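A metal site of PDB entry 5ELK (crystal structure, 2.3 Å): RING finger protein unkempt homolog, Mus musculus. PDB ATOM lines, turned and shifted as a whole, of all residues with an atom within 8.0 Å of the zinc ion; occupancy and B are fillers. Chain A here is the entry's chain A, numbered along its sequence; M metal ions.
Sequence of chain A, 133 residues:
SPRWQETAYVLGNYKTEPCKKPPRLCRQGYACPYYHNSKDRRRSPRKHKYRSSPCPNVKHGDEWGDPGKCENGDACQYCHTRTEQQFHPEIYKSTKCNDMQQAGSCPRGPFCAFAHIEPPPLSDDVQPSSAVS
The side-chain sulfur of Cys 32 sits close to the backbone NH of Tyr 34 (3.7 Å).
A ring nitrogen (ND1) of His 36 sits at hydrogen-bond distance from the side-chain carboxylate (OD2) of Asp 40 (3.0 Å).
The backbone carbonyl oxygen of Tyr 35 lies within hydrogen-bond range of the backbone NH of Cys 19.
The side-chain sulfur (SG) of Cys 19 lies close to the backbone carbonyl oxygen (O) of Lys 21, 3.4 Å away.
NZ of Lys 15 is in hydrogen-bond range of O of Cys 32, 2.8 Å away.
The backbone carbonyl oxygen of Tyr 34 lies close to a ring nitrogen (ND1) of His 36.
Within 4 Å of the zinc ion: Cys 19, Cys 26, Cys 32 and His 36.
The nearest printed residue that does not touch the zinc ion is Tyr 34 (4.6 Å).
The zinc ion is bound by a ring nitrogen (NE2) of His 36 (2.0 Å), the side-chain sulfur of Cys 19 (2.3 Å), the side-chain sulfur of Cys 26 (2.3 Å) and the side-chain sulfur of Cys 32 (2.3 Å).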
ATOM      1  N   LYS A  15       3.315   9.783  13.808  1.00  0.00           N
ATOM      2  CA  LYS A  15       2.815  11.145  13.633  1.00  0.00           C
ATOM      3  C   LYS A  15       1.301  11.291  13.787  1.00  0.00           C
ATOM      4  O   LYS A  15       0.662  12.093  13.118  1.00  0.00           O
ATOM      5  CB  LYS A  15       3.298  11.723  12.305  1.00  0.00           C
ATOM      6  CG  LYS A  15       4.760  12.059  12.370  1.00  0.00           C
ATOM      7  CD  LYS A  15       5.317  12.479  11.040  1.00  0.00           C
ATOM      8  CE  LYS A  15       6.795  12.786  11.144  1.00  0.00           C
ATOM      9  NZ  LYS A  15       7.091  13.813  12.189  1.00  0.00           N
ATOM     10  N   GLU A  17       0.206  11.977  16.797  1.00  0.00           N
ATOM     11  CA  GLU A  17       0.135  12.859  17.954  1.00  0.00           C
ATOM     12  C   GLU A  17       1.262  13.903  17.939  1.00  0.00           C
ATOM     13  O   GLU A  17       2.255  13.734  17.220  1.00  0.00           O
ATOM     14  CB  GLU A  17       0.178  12.028  19.235  1.00  0.00           C
ATOM     15  CG  GLU A  17      -1.129  11.293  19.535  1.00  0.00           C
ATOM     16  CD  GLU A  17      -1.033  10.334  20.708  1.00  0.00           C
ATOM     17  OE1 GLU A  17      -0.124   9.484  20.713  1.00  0.00           O
ATOM     18  OE2 GLU A  17      -1.877  10.416  21.629  1.00  0.00           O
ATOM     19  N   PRO A  18       1.098  14.991  18.707  1.00  0.00           N
ATOM     20  CA  PRO A  18       2.027  16.119  18.657  1.00  0.00           C
ATOM     21  C   PRO A  18       3.233  16.009  19.582  1.00  0.00           C
ATOM     22  O   PRO A  18       3.120  15.553  20.718  1.00  0.00           O
ATOM     23  CB  PRO A  18       1.166  17.305  19.082  1.00  0.00           C
ATOM     24  CG  PRO A  18       0.120  16.705  19.968  1.00  0.00           C
ATOM     25  CD  PRO A  18      -0.126  15.309  19.467  1.00  0.00           C
ATOM     26  N   CYS A  19       4.382  16.469  19.088  1.00  0.00           N
ATOM     27  CA  CYS A  19       5.611  16.455  19.847  1.00  0.00           C
ATOM     28  C   CYS A  19       5.489  17.320  21.102  1.00  0.00           C
ATOM     29  O   CYS A  19       5.052  18.471  21.013  1.00  0.00           O
ATOM     30  CB  CYS A  19       6.762  16.966  18.992  1.00  0.00           C
ATOM     31  SG  CYS A  19       8.376  16.619  19.653  1.00  0.00           S
ATOM     32  N   LYS A  20       5.862  16.766  22.254  1.00  0.00           N
ATOM     33  CA  LYS A  20       5.857  17.504  23.521  1.00  0.00           C
ATOM     34  C   LYS A  20       6.716  18.759  23.454  1.00  0.00           C
ATOM     35  O   LYS A  20       6.307  19.827  23.928  1.00  0.00           O
ATOM     36  CB  LYS A  20       6.350  16.622  24.670  1.00  0.00           C
ATOM     37  CG  LYS A  20       5.297  15.715  25.306  1.00  0.00           C
ATOM     38  CD  LYS A  20       4.044  16.479  25.729  1.00  0.00           C
ATOM     39  CE  LYS A  20       2.968  16.471  24.638  1.00  0.00           C
ATOM     40  NZ  LYS A  20       2.457  17.837  24.292  1.00  0.00           N
ATOM     41  N   LYS A  21       7.900  18.634  22.872  1.00  0.00           N
ATOM     42  CA  LYS A  21       8.839  19.734  22.794  1.00  0.00           C
ATOM     43  C   LYS A  21       8.686  20.485  21.471  1.00  0.00           C
ATOM     44  O   LYS A  21       8.950  19.924  20.409  1.00  0.00           O
ATOM     45  CB  LYS A  21      10.269  19.202  22.931  1.00  0.00           C
ATOM     46  CG  LYS A  21      10.999  19.723  24.159  1.00  0.00           C
ATOM     47  CD  LYS A  21      12.497  19.474  24.086  1.00  0.00           C
ATOM     48  CE  LYS A  21      13.170  19.772  25.412  1.00  0.00           C
ATOM     49  NZ  LYS A  21      12.745  21.081  25.971  1.00  0.00           N
ATOM     50  N   PRO A  22       8.243  21.753  21.533  1.00  0.00           N
ATOM     51  CA  PRO A  22       8.257  22.590  20.319  1.00  0.00           C
ATOM     52  C   PRO A  22       9.607  23.267  19.979  1.00  0.00           C
ATOM     53  O   PRO A  22       9.636  23.988  18.976  1.00  0.00           O
ATOM     54  CB  PRO A  22       7.209  23.658  20.636  1.00  0.00           C
ATOM     55  CG  PRO A  22       7.308  23.834  22.101  1.00  0.00           C
ATOM     56  CD  PRO A  22       7.558  22.441  22.648  1.00  0.00           C
ATOM     57  N   PRO A  23      10.683  23.056  20.765  1.00  0.00           N
ATOM     58  CA  PRO A  23      11.885  23.761  20.291  1.00  0.00           C
ATOM     59  C   PRO A  23      12.448  23.206  18.984  1.00  0.00           C
ATOM     60  O   PRO A  23      12.014  22.156  18.521  1.00  0.00           O
ATOM     61  CB  PRO A  23      12.890  23.561  21.439  1.00  0.00           C
ATOM     62  CG  PRO A  23      12.069  23.207  22.619  1.00  0.00           C
ATOM     63  CD  PRO A  23      10.945  22.400  22.058  1.00  0.00           C
ATOM     64  N   LEU A  25      15.072  21.831  18.541  1.00  0.00           N
ATOM     65  CA  LEU A  25      15.979  20.728  18.825  1.00  0.00           C
ATOM     66  C   LEU A  25      15.557  19.493  18.076  1.00  0.00           C
ATOM     67  O   LEU A  25      16.384  18.687  17.643  1.00  0.00           O
ATOM     68  CB  LEU A  25      15.985  20.435  20.317  1.00  0.00           C
ATOM     69  CG  LEU A  25      16.362  21.611  21.190  1.00  0.00           C
ATOM     70  CD1 LEU A  25      16.602  21.105  22.608  1.00  0.00           C
ATOM     71  CD2 LEU A  25      17.577  22.350  20.611  1.00  0.00           C
ATOM     72  N   CYS A  26      14.247  19.326  17.947  1.00  0.00           N
ATOM     73  CA  CYS A  26      13.694  18.283  17.122  1.00  0.00           C
ATOM     74  C   CYS A  26      14.215  18.511  15.712  1.00  0.00           C
ATOM     75  O   CYS A  26      14.176  19.636  15.209  1.00  0.00           O
ATOM     76  CB  CYS A  26      12.176  18.345  17.167  1.00  0.00           C
ATOM     77  SG  CYS A  26      11.339  16.785  16.904  1.00  0.00           S
ATOM     78  N   ARG A  27      14.733  17.464  15.068  1.00  0.00           N
ATOM     79  CA  ARG A  27      15.167  17.558  13.678  1.00  0.00           C
ATOM     80  C   ARG A  27      13.980  17.868  12.784  1.00  0.00           C
ATOM     81  O   ARG A  27      14.146  18.194  11.615  1.00  0.00           O
ATOM     82  CB  ARG A  27      15.852  16.261  13.217  1.00  0.00           C
ATOM     83  CG  ARG A  27      17.373  16.298  13.335  1.00  0.00           C
ATOM     84  CD  ARG A  27      18.010  17.013  12.137  1.00  0.00           C
ATOM     85  NE  ARG A  27      19.430  17.305  12.361  1.00  0.00           N
ATOM     86  CZ  ARG A  27      19.886  18.439  12.883  1.00  0.00           C
ATOM     87  NH1 ARG A  27      19.055  19.406  13.254  1.00  0.00           N
ATOM     88  NH2 ARG A  27      21.195  18.613  13.039  1.00  0.00           N
ATOM     89  N   GLN A  28      12.779  17.742  13.356  1.00  0.00           N
ATOM     90  CA  GLN A  28      11.569  18.282  12.741  1.00  0.00           C
ATOM     91  C   GLN A  28      11.232  17.526  11.468  1.00  0.00           C
ATOM     92  O   GLN A  28      10.732  18.105  10.502  1.00  0.00           O
ATOM     93  CB  GLN A  28      11.752  19.769  12.417  1.00  0.00           C
ATOM     94  CG  GLN A  28      10.453  20.544  12.201  1.00  0.00           C
ATOM     95  CD  GLN A  28       9.787  20.914  13.512  1.00  0.00           C
ATOM     96  OE1 GLN A  28      10.124  20.375  14.554  1.00  0.00           O
ATOM     97  NE2 GLN A  28       8.844  21.841  13.447  1.00  0.00           N
ATOM     98  N   GLY A  29      11.500  16.221  11.461  1.00  0.00           N
ATOM     99  CA  GLY A  29      11.230  15.441  10.265  1.00  0.00           C
ATOM    100  C   GLY A  29      10.931  13.993  10.571  1.00  0.00           C
ATOM    101  O   GLY A  29      10.290  13.699  11.581  1.00  0.00           O
ATOM    102  N   ALA A  31      12.625  11.756  11.730  1.00  0.00           N
ATOM    103  CA  ALA A  31      13.332  11.264  12.910  1.00  0.00           C
ATOM    104  C   ALA A  31      12.469  11.336  14.157  1.00  0.00           C
ATOM    105  O   ALA A  31      12.789  10.713  15.171  1.00  0.00           O
ATOM    106  CB  ALA A  31      14.618  12.068  13.127  1.00  0.00           C
ATOM    107  N   CYS A  32      11.389  12.118  14.098  1.00  0.00           N
ATOM    108  CA  CYS A  32      10.502  12.291  15.248  1.00  0.00           C
ATOM    109  C   CYS A  32       9.100  11.742  14.974  1.00  0.00           C
ATOM    110  O   CYS A  32       8.384  12.268  14.130  1.00  0.00           O
ATOM    111  CB  CYS A  32      10.394  13.756  15.652  1.00  0.00           C
ATOM    112  SG  CYS A  32       9.348  13.960  17.095  1.00  0.00           S
ATOM    113  N   PRO A  33       8.682  10.699  15.718  1.00  0.00           N
ATOM    114  CA  PRO A  33       7.409  10.016  15.437  1.00  0.00           C
ATOM    115  C   PRO A  33       6.167  10.793  15.872  1.00  0.00           C
ATOM    116  O   PRO A  33       5.080  10.216  15.925  1.00  0.00           O
ATOM    117  CB  PRO A  33       7.538   8.721  16.238  1.00  0.00           C
ATOM    118  CG  PRO A  33       8.398   9.109  17.422  1.00  0.00           C
ATOM    119  CD  PRO A  33       9.372  10.118  16.893  1.00  0.00           C
ATOM    120  N   TYR A  34       6.330  12.082  16.165  1.00  0.00           N
ATOM    121  CA  TYR A  34       5.201  12.923  16.550  1.00  0.00           C
ATOM    122  C   TYR A  34       5.136  14.067  15.539  1.00  0.00           C
ATOM    123  O   TYR A  34       6.103  14.300  14.813  1.00  0.00           O
ATOM    124  CB  TYR A  34       5.384  13.427  17.983  1.00  0.00           C
ATOM    125  CG  TYR A  34       5.471  12.293  19.000  1.00  0.00           C
ATOM    126  CD1 TYR A  34       4.329  11.585  19.375  1.00  0.00           C
ATOM    127  CD2 TYR A  34       6.681  11.925  19.573  1.00  0.00           C
ATOM    128  CE1 TYR A  34       4.402  10.551  20.303  1.00  0.00           C
ATOM    129  CE2 TYR A  34       6.760  10.894  20.493  1.00  0.00           C
ATOM    130  CZ  TYR A  34       5.622  10.202  20.863  1.00  0.00           C
ATOM    131  OH  TYR A  34       5.694   9.178  21.781  1.00  0.00           O
ATOM    132  N   TYR A  35       3.988  14.748  15.461  1.00  0.00           N
ATOM    133  CA  TYR A  35       3.823  15.776  14.441  1.00  0.00           C
ATOM    134  C   TYR A  35       4.016  17.161  15.016  1.00  0.00           C
ATOM    135  O   TYR A  35       3.746  17.423  16.187  1.00  0.00           O
ATOM    136  CB  TYR A  35       2.471  15.665  13.704  1.00  0.00           C
ATOM    137  CG  TYR A  35       1.239  16.084  14.494  1.00  0.00           C
ATOM    138  CD1 TYR A  35       0.935  17.423  14.703  1.00  0.00           C
ATOM    139  CD2 TYR A  35       0.355  15.139  14.994  1.00  0.00           C
ATOM    140  CE1 TYR A  35      -0.191  17.799  15.400  1.00  0.00           C
ATOM    141  CE2 TYR A  35      -0.769  15.501  15.687  1.00  0.00           C
ATOM    142  CZ  TYR A  35      -1.041  16.824  15.888  1.00  0.00           C
ATOM    143  OH  TYR A  35      -2.181  17.175  16.591  1.00  0.00           O
ATOM    144  N   HIS A  36       4.498  18.052  14.150  1.00  0.00           N
ATOM    145  CA  HIS A  36       4.945  19.382  14.556  1.00  0.00           C
ATOM    146  C   HIS A  36       4.089  20.447  13.888  1.00  0.00           C
ATOM    147  O   HIS A  36       3.970  21.563  14.393  1.00  0.00           O
ATOM    148  CB  HIS A  36       6.415  19.530  14.168  1.00  0.00           C
ATOM    149  CG  HIS A  36       7.294  18.477  14.767  1.00  0.00           C
ATOM    150  ND1 HIS A  36       7.309  17.179  14.317  1.00  0.00           N
ATOM    151  CD2 HIS A  36       8.173  18.531  15.798  1.00  0.00           C
ATOM    152  CE1 HIS A  36       8.162  16.469  15.029  1.00  0.00           C
ATOM    153  NE2 HIS A  36       8.713  17.265  15.932  1.00  0.00           N
ATOM    154  N   ASP A  40       2.608  17.828   8.600  1.00  0.00           N
ATOM    155  CA  ASP A  40       3.401  16.722   9.158  1.00  0.00           C
ATOM    156  C   ASP A  40       2.442  15.723   9.803  1.00  0.00           C
ATOM    157  O   ASP A  40       2.805  14.589  10.112  1.00  0.00           O
ATOM    158  CB  ASP A  40       4.334  17.312  10.222  1.00  0.00           C
ATOM    159  CG  ASP A  40       5.421  16.365  10.661  1.00  0.00           C
ATOM    160  OD1 ASP A  40       5.894  15.579   9.821  1.00  0.00           O
ATOM    161  OD2 ASP A  40       5.814  16.425  11.835  1.00  0.00           O
HETATM  162 ZN    ZN M   1       9.227  16.232  17.590  1.00  0.00          ZN
